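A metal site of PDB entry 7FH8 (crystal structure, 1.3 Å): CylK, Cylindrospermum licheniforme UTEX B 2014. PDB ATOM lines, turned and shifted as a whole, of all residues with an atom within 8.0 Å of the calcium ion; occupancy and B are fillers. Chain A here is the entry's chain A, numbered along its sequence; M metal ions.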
ATOM      1  N   ASP A 115       6.342   5.466  -9.637  1.00  0.00           N
ATOM      2  CA  ASP A 115       5.817   5.256  -8.297  1.00  0.00           C
ATOM      3  C   ASP A 115       5.982   3.777  -7.933  1.00  0.00           C
ATOM      4  O   ASP A 115       5.298   2.936  -8.525  1.00  0.00           O
ATOM      5  CB  ASP A 115       4.358   5.675  -8.228  1.00  0.00           C
ATOM      6  CG  ASP A 115       3.825   5.730  -6.818  1.00  0.00           C
ATOM      7  OD1 ASP A 115       4.243   4.877  -5.994  1.00  0.00           O
ATOM      8  OD2 ASP A 115       2.987   6.622  -6.521  1.00  0.00           O
ATOM      9  N   PRO A 116       6.847   3.432  -6.971  1.00  0.00           N
ATOM     10  CA  PRO A 116       7.055   2.015  -6.653  1.00  0.00           C
ATOM     11  C   PRO A 116       5.859   1.345  -6.007  1.00  0.00           C
ATOM     12  O   PRO A 116       5.829   0.108  -5.929  1.00  0.00           O
ATOM     13  CB  PRO A 116       8.271   2.050  -5.711  1.00  0.00           C
ATOM     14  CG  PRO A 116       8.185   3.407  -5.059  1.00  0.00           C
ATOM     15  CD  PRO A 116       7.684   4.325  -6.151  1.00  0.00           C
ATOM     16  N   GLY A 117       4.876   2.112  -5.546  1.00  0.00           N
ATOM     17  CA  GLY A 117       3.676   1.562  -4.969  1.00  0.00           C
ATOM     18  C   GLY A 117       2.510   1.414  -5.912  1.00  0.00           C
ATOM     19  O   GLY A 117       1.452   0.934  -5.499  1.00  0.00           O
ATOM     20  N   TRP A 160      15.737   2.649  -1.304  1.00  0.00           N
ATOM     21  CA  TRP A 160      15.995   1.581  -0.342  1.00  0.00           C
ATOM     22  C   TRP A 160      15.063   0.388  -0.555  1.00  0.00           C
ATOM     23  O   TRP A 160      15.399  -0.730  -0.157  1.00  0.00           O
ATOM     24  CB  TRP A 160      15.817   2.109   1.089  1.00  0.00           C
ATOM     25  CG  TRP A 160      14.458   2.699   1.323  1.00  0.00           C
ATOM     26  CD1 TRP A 160      14.096   4.017   1.181  1.00  0.00           C
ATOM     27  CD2 TRP A 160      13.257   1.991   1.690  1.00  0.00           C
ATOM     28  NE1 TRP A 160      12.752   4.175   1.450  1.00  0.00           N
ATOM     29  CE2 TRP A 160      12.216   2.945   1.761  1.00  0.00           C
ATOM     30  CE3 TRP A 160      12.969   0.647   1.962  1.00  0.00           C
ATOM     31  CZ2 TRP A 160      10.907   2.602   2.094  1.00  0.00           C
ATOM     32  CZ3 TRP A 160      11.678   0.305   2.308  1.00  0.00           C
ATOM     33  CH2 TRP A 160      10.657   1.273   2.364  1.00  0.00           C
ATOM     34  N   GLN A 161      13.900   0.608  -1.162  1.00  0.00           N
ATOM     35  CA  GLN A 161      12.870  -0.416  -1.259  1.00  0.00           C
ATOM     36  C   GLN A 161      13.065  -1.330  -2.455  1.00  0.00           C
ATOM     37  O   GLN A 161      12.997  -2.556  -2.306  1.00  0.00           O
ATOM     38  CB  GLN A 161      11.500   0.241  -1.330  1.00  0.00           C
ATOM     39  CG  GLN A 161      10.346  -0.707  -1.135  1.00  0.00           C
ATOM     40  CD  GLN A 161       9.040   0.053  -1.213  1.00  0.00           C
ATOM     41  OE1 GLN A 161       8.724   0.635  -2.262  1.00  0.00           O
ATOM     42  NE2 GLN A 161       8.284   0.077  -0.119  1.00  0.00           N
ATOM     43  N   HIS A 254       2.781  10.823  11.118  1.00  0.00           N
ATOM     44  CA  HIS A 254       3.203  10.242   9.852  1.00  0.00           C
ATOM     45  C   HIS A 254       1.984   9.818   9.046  1.00  0.00           C
ATOM     46  O   HIS A 254       1.097   9.144   9.583  1.00  0.00           O
ATOM     47  CB  HIS A 254       4.082   9.022  10.113  1.00  0.00           C
ATOM     48  CG  HIS A 254       4.472   8.275   8.875  1.00  0.00           C
ATOM     49  ND1 HIS A 254       3.647   7.357   8.267  1.00  0.00           N
ATOM     50  CD2 HIS A 254       5.603   8.332   8.117  1.00  0.00           C
ATOM     51  CE1 HIS A 254       4.257   6.869   7.193  1.00  0.00           C
ATOM     52  NE2 HIS A 254       5.437   7.440   7.089  1.00  0.00           N
ATOM     53  N   ILE A 255       1.955  10.206   7.769  1.00  0.00           N
ATOM     54  CA  ILE A 255       0.908   9.813   6.840  1.00  0.00           C
ATOM     55  C   ILE A 255       1.580   9.198   5.604  1.00  0.00           C
ATOM     56  O   ILE A 255       2.345   9.878   4.910  1.00  0.00           O
ATOM     57  CB  ILE A 255       0.011  10.998   6.439  1.00  0.00           C
ATOM     58  CG1 ILE A 255      -0.688  11.569   7.679  1.00  0.00           C
ATOM     59  CG2 ILE A 255      -0.996  10.563   5.399  1.00  0.00           C
ATOM     60  CD1 ILE A 255      -1.446  12.865   7.408  1.00  0.00           C
ATOM     61  N   GLY A 256       1.319   7.925   5.336  1.00  0.00           N
ATOM     62  CA  GLY A 256       1.934   7.332   4.168  1.00  0.00           C
ATOM     63  C   GLY A 256       1.374   5.991   3.774  1.00  0.00           C
ATOM     64  O   GLY A 256       0.860   5.235   4.607  1.00  0.00           O
ATOM     65  N   THR A 257       1.487   5.714   2.474  1.00  0.00           N
ATOM     66  CA  THR A 257       1.201   4.431   1.848  1.00  0.00           C
ATOM     67  C   THR A 257       2.440   3.980   1.095  1.00  0.00           C
ATOM     68  O   THR A 257       3.442   4.701   1.020  1.00  0.00           O
ATOM     69  CB  THR A 257       0.017   4.518   0.863  1.00  0.00           C
ATOM     70  OG1 THR A 257       0.443   5.153  -0.359  1.00  0.00           O
ATOM     71  CG2 THR A 257      -1.198   5.248   1.483  1.00  0.00           C
ATOM     72  N   ALA A 258       2.355   2.801   0.482  1.00  0.00           N
ATOM     73  CA  ALA A 258       3.419   2.311  -0.393  1.00  0.00           C
ATOM     74  C   ALA A 258       3.671   3.215  -1.598  1.00  0.00           C
ATOM     75  O   ALA A 258       4.737   3.112  -2.228  1.00  0.00           O
ATOM     76  CB  ALA A 258       3.076   0.897  -0.881  1.00  0.00           C
ATOM     77  N   ALA A 259       2.727   4.065  -1.978  1.00  0.00           N
ATOM     78  CA  ALA A 259       2.845   4.908  -3.162  1.00  0.00           C
ATOM     79  C   ALA A 259       3.391   6.290  -2.775  1.00  0.00           C
ATOM     80  O   ALA A 259       3.768   6.526  -1.625  1.00  0.00           O
ATOM     81  CB  ALA A 259       1.501   5.002  -3.875  1.00  0.00           C
ATOM     82  N   ASN A 260       3.438   7.213  -3.729  1.00  0.00           N
ATOM     83  CA  ASN A 260       3.833   8.583  -3.405  1.00  0.00           C
ATOM     84  C   ASN A 260       2.690   9.307  -2.724  1.00  0.00           C
ATOM     85  O   ASN A 260       1.591   9.402  -3.271  1.00  0.00           O
ATOM     86  CB  ASN A 260       4.249   9.338  -4.673  1.00  0.00           C
ATOM     87  CG  ASN A 260       5.616   8.943  -5.131  1.00  0.00           C
ATOM     88  OD1 ASN A 260       6.524   8.858  -4.322  1.00  0.00           O
ATOM     89  ND2 ASN A 260       5.773   8.689  -6.418  1.00  0.00           N
ATOM     90  N   ASP A 261       2.934   9.834  -1.522  1.00  0.00           N
ATOM     91  CA  ASP A 261       1.926  10.563  -0.761  1.00  0.00           C
ATOM     92  C   ASP A 261       2.440  11.941  -0.407  1.00  0.00           C
ATOM     93  O   ASP A 261       3.562  12.059   0.119  1.00  0.00           O
ATOM     94  CB  ASP A 261       1.594   9.853   0.554  1.00  0.00           C
ATOM     95  CG  ASP A 261       1.490   8.362   0.393  1.00  0.00           C
ATOM     96  OD1 ASP A 261       0.477   7.897  -0.176  1.00  0.00           O
ATOM     97  OD2 ASP A 261       2.415   7.662   0.813  1.00  0.00           O
ATOM     98  N   TYR A 262       1.618  12.965  -0.647  1.00  0.00           N
ATOM     99  CA  TYR A 262       2.006  14.359  -0.419  1.00  0.00           C
ATOM    100  C   TYR A 262       0.926  15.099   0.351  1.00  0.00           C
ATOM    101  O   TYR A 262      -0.256  15.038  -0.008  1.00  0.00           O
ATOM    102  CB  TYR A 262       2.212  15.107  -1.743  1.00  0.00           C
ATOM    103  CG  TYR A 262       3.116  14.391  -2.712  1.00  0.00           C
ATOM    104  CD1 TYR A 262       4.490  14.592  -2.685  1.00  0.00           C
ATOM    105  CD2 TYR A 262       2.598  13.502  -3.648  1.00  0.00           C
ATOM    106  CE1 TYR A 262       5.343  13.912  -3.550  1.00  0.00           C
ATOM    107  CE2 TYR A 262       3.425  12.836  -4.521  1.00  0.00           C
ATOM    108  CZ  TYR A 262       4.792  13.050  -4.478  1.00  0.00           C
ATOM    109  OH  TYR A 262       5.617  12.362  -5.347  1.00  0.00           O
ATOM    110  N   THR A 280      -2.178  11.643  -3.600  1.00  0.00           N
ATOM    111  CA  THR A 280      -1.621  10.330  -3.315  1.00  0.00           C
ATOM    112  C   THR A 280      -1.748   9.403  -4.518  1.00  0.00           C
ATOM    113  O   THR A 280      -2.783   9.380  -5.192  1.00  0.00           O
ATOM    114  CB  THR A 280      -2.260   9.674  -2.086  1.00  0.00           C
ATOM    115  OG1 THR A 280      -1.677   8.378  -1.873  1.00  0.00           O
ATOM    116  CG2 THR A 280      -3.779   9.512  -2.269  1.00  0.00           C
ATOM    117  N   GLY A 281      -0.688   8.636  -4.780  1.00  0.00           N
ATOM    118  CA  GLY A 281      -0.749   7.543  -5.728  1.00  0.00           C
ATOM    119  C   GLY A 281      -1.267   6.246  -5.155  1.00  0.00           C
ATOM    120  O   GLY A 281      -1.324   5.241  -5.874  1.00  0.00           O
ATOM    121  N   GLY A 282      -1.628   6.241  -3.861  1.00  0.00           N
ATOM    122  CA  GLY A 282      -2.092   5.044  -3.200  1.00  0.00           C
ATOM    123  C   GLY A 282      -3.502   5.165  -2.685  1.00  0.00           C
ATOM    124  O   GLY A 282      -4.286   6.003  -3.151  1.00  0.00           O
ATOM    125  N   LEU A 284      -5.053   6.119   0.447  1.00  0.00           N
ATOM    126  CA  LEU A 284      -4.719   6.812   1.685  1.00  0.00           C
ATOM    127  C   LEU A 284      -5.980   7.123   2.492  1.00  0.00           C
ATOM    128  O   LEU A 284      -6.135   6.636   3.618  1.00  0.00           O
ATOM    129  CB  LEU A 284      -3.906   8.067   1.359  1.00  0.00           C
ATOM    130  CG  LEU A 284      -3.200   8.849   2.473  1.00  0.00           C
ATOM    131  CD1 LEU A 284      -2.221   9.832   1.842  1.00  0.00           C
ATOM    132  CD2 LEU A 284      -4.158   9.608   3.383  1.00  0.00           C
ATOM    133  N   THR A 631       8.589  13.861   2.618  1.00  0.00           N
ATOM    134  CA  THR A 631       9.922  13.336   2.893  1.00  0.00           C
ATOM    135  C   THR A 631      10.161  12.027   2.137  1.00  0.00           C
ATOM    136  O   THR A 631       9.235  11.232   1.911  1.00  0.00           O
ATOM    137  CB  THR A 631      10.134  13.116   4.404  1.00  0.00           C
ATOM    138  OG1 THR A 631      11.491  12.728   4.640  1.00  0.00           O
ATOM    139  CG2 THR A 631       9.224  12.019   4.960  1.00  0.00           C
ATOM    140  N   THR A 638       8.486   4.511  10.114  1.00  0.00           N
ATOM    141  CA  THR A 638       9.194   3.960   8.962  1.00  0.00           C
ATOM    142  C   THR A 638       8.526   4.345   7.645  1.00  0.00           C
ATOM    143  O   THR A 638       7.307   4.195   7.478  1.00  0.00           O
ATOM    144  CB  THR A 638       9.207   2.431   9.100  1.00  0.00           C
ATOM    145  OG1 THR A 638       9.792   2.047  10.348  1.00  0.00           O
ATOM    146  CG2 THR A 638      10.013   1.809   7.969  1.00  0.00           C
ATOM    147  N   ASN A 639       9.329   4.830   6.701  1.00  0.00           N
ATOM    148  CA  ASN A 639       8.814   5.143   5.369  1.00  0.00           C
ATOM    149  C   ASN A 639       8.182   3.913   4.742  1.00  0.00           C
ATOM    150  O   ASN A 639       8.749   2.821   4.749  1.00  0.00           O
ATOM    151  CB  ASN A 639       9.951   5.674   4.494  1.00  0.00           C
ATOM    152  CG  ASN A 639       9.464   6.260   3.192  1.00  0.00           C
ATOM    153  OD1 ASN A 639       9.021   5.531   2.308  1.00  0.00           O
ATOM    154  ND2 ASN A 639       9.519   7.591   3.061  1.00  0.00           N
ATOM    155  N   ALA A 640       6.961   4.075   4.219  1.00  0.00           N
ATOM    156  CA  ALA A 640       6.216   2.976   3.595  1.00  0.00           C
ATOM    157  C   ALA A 640       6.466   2.852   2.108  1.00  0.00           C
ATOM    158  O   ALA A 640       6.080   1.836   1.512  1.00  0.00           O
ATOM    159  CB  ALA A 640       4.708   3.146   3.848  1.00  0.00           C
ATOM    160  N   GLY A 641       7.070   3.857   1.488  1.00  0.00           N
ATOM    161  CA  GLY A 641       7.360   3.808   0.072  1.00  0.00           C
ATOM    162  C   GLY A 641       7.507   5.200  -0.479  1.00  0.00           C
ATOM    163  O   GLY A 641       6.665   6.054  -0.237  1.00  0.00           O
ATOM    164  N   SER A 642       8.623   5.415  -1.197  1.00  0.00           N
ATOM    165  CA  SER A 642       8.934   6.664  -1.875  1.00  0.00           C
ATOM    166  C   SER A 642       8.626   7.870  -0.982  1.00  0.00           C
ATOM    167  O   SER A 642       9.161   7.969   0.122  1.00  0.00           O
ATOM    168  CB  SER A 642       8.236   6.689  -3.228  1.00  0.00           C
ATOM    169  OG  SER A 642       8.794   7.679  -4.060  1.00  0.00           O
ATOM    170  N   TYR A 643       7.773   8.796  -1.441  1.00  0.00           N
ATOM    171  CA  TYR A 643       7.387   9.923  -0.608  1.00  0.00           C
ATOM    172  C   TYR A 643       6.305   9.542   0.406  1.00  0.00           C
ATOM    173  O   TYR A 643       5.281   8.951   0.042  1.00  0.00           O
ATOM    174  CB  TYR A 643       6.904  11.109  -1.453  1.00  0.00           C
ATOM    175  CG  TYR A 643       8.062  11.891  -2.027  1.00  0.00           C
ATOM    176  CD1 TYR A 643       8.781  11.430  -3.131  1.00  0.00           C
ATOM    177  CD2 TYR A 643       8.532  13.041  -1.392  1.00  0.00           C
ATOM    178  CE1 TYR A 643       9.875  12.123  -3.617  1.00  0.00           C
ATOM    179  CE2 TYR A 643       9.618  13.749  -1.875  1.00  0.00           C
ATOM    180  CZ  TYR A 643      10.296  13.286  -2.982  1.00  0.00           C
ATOM    181  OH  TYR A 643      11.384  13.981  -3.459  1.00  0.00           O
ATOM    182  N   ASP A 644       6.539   9.902   1.663  1.00  0.00           N
ATOM    183  CA  ASP A 644       5.537   9.924   2.712  1.00  0.00           C
ATOM    184  C   ASP A 644       5.395  11.369   3.183  1.00  0.00           C
ATOM    185  O   ASP A 644       6.180  12.243   2.803  1.00  0.00           O
ATOM    186  CB  ASP A 644       5.952   9.038   3.899  1.00  0.00           C
ATOM    187  CG  ASP A 644       5.745   7.550   3.643  1.00  0.00           C
ATOM    188  OD1 ASP A 644       5.256   7.161   2.563  1.00  0.00           O
ATOM    189  OD2 ASP A 644       6.109   6.770   4.549  1.00  0.00           O
ATOM    190  N   SER A 645       4.396  11.620   4.022  1.00  0.00           N
ATOM    191  CA  SER A 645       4.132  12.967   4.506  1.00  0.00           C
ATOM    192  C   SER A 645       4.101  13.006   6.027  1.00  0.00           C
ATOM    193  O   SER A 645       4.038  11.973   6.701  1.00  0.00           O
ATOM    194  CB  SER A 645       2.844  13.534   3.908  1.00  0.00           C
ATOM    195  OG  SER A 645       3.020  13.692   2.514  1.00  0.00           O
HETATM  196 CA    CA M   1       4.534   6.720   0.488  1.00  0.00          CA
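The side-chain carboxylate (OD2) of Asp 644 sits at hydrogen-bond distance from a ring nitrogen (NE2) of His 254 (2.7 Å). O of Asp 261 lies within hydrogen-bond range of OG of Ser 645. The backbone carbonyl oxygen (O) of Asp 644 is in hydrogen-bond range of the backbone NH (N) of Thr 631, at 2.9 Å. The side-chain carboxylate (OD1) of Asp 261 lies within hydrogen-bond range of the side-chain hydroxyl (OG1) of Thr 280 (2.8 Å). The backbone NH of Ala 259 is in hydrogen-bond range of the side-chain hydroxyl of Thr 257, at 3.0 Å. OD1 of Asn 260 is in hydrogen-bond range of N of Tyr 643 (3.1 Å). The side-chain carboxylate (OD2) of Asp 644 lies within hydrogen-bond range of the backbone NH (N) of Ala 640 (2.8 Å). The side-chain amide oxygen (OD1) of Asn 639 lies within hydrogen-bond range of the backbone NH (N) of Gly 641 (2.7 Å).
Of the 27 residues printed, 6 come within 4 Å of the calcium ion. The nearest printed residue that does not touch the calcium ion is Ala 258 (4.2 Å).
The calcium ion is bound by the side-chain carboxylate of Asp 644 (2.2 Å), the backbone carbonyl oxygen of Ala 259 (2.3 Å), the side-chain carboxylate of Asp 261 (2.3 Å), the backbone carbonyl oxygen of Gly 641 (2.3 Å), the backbone carbonyl oxygen of Thr 257 (2.4 Å) and the backbone carbonyl oxygen of Tyr 643 (2.4 Å). The calcium ion has six donor atoms within binding distance.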
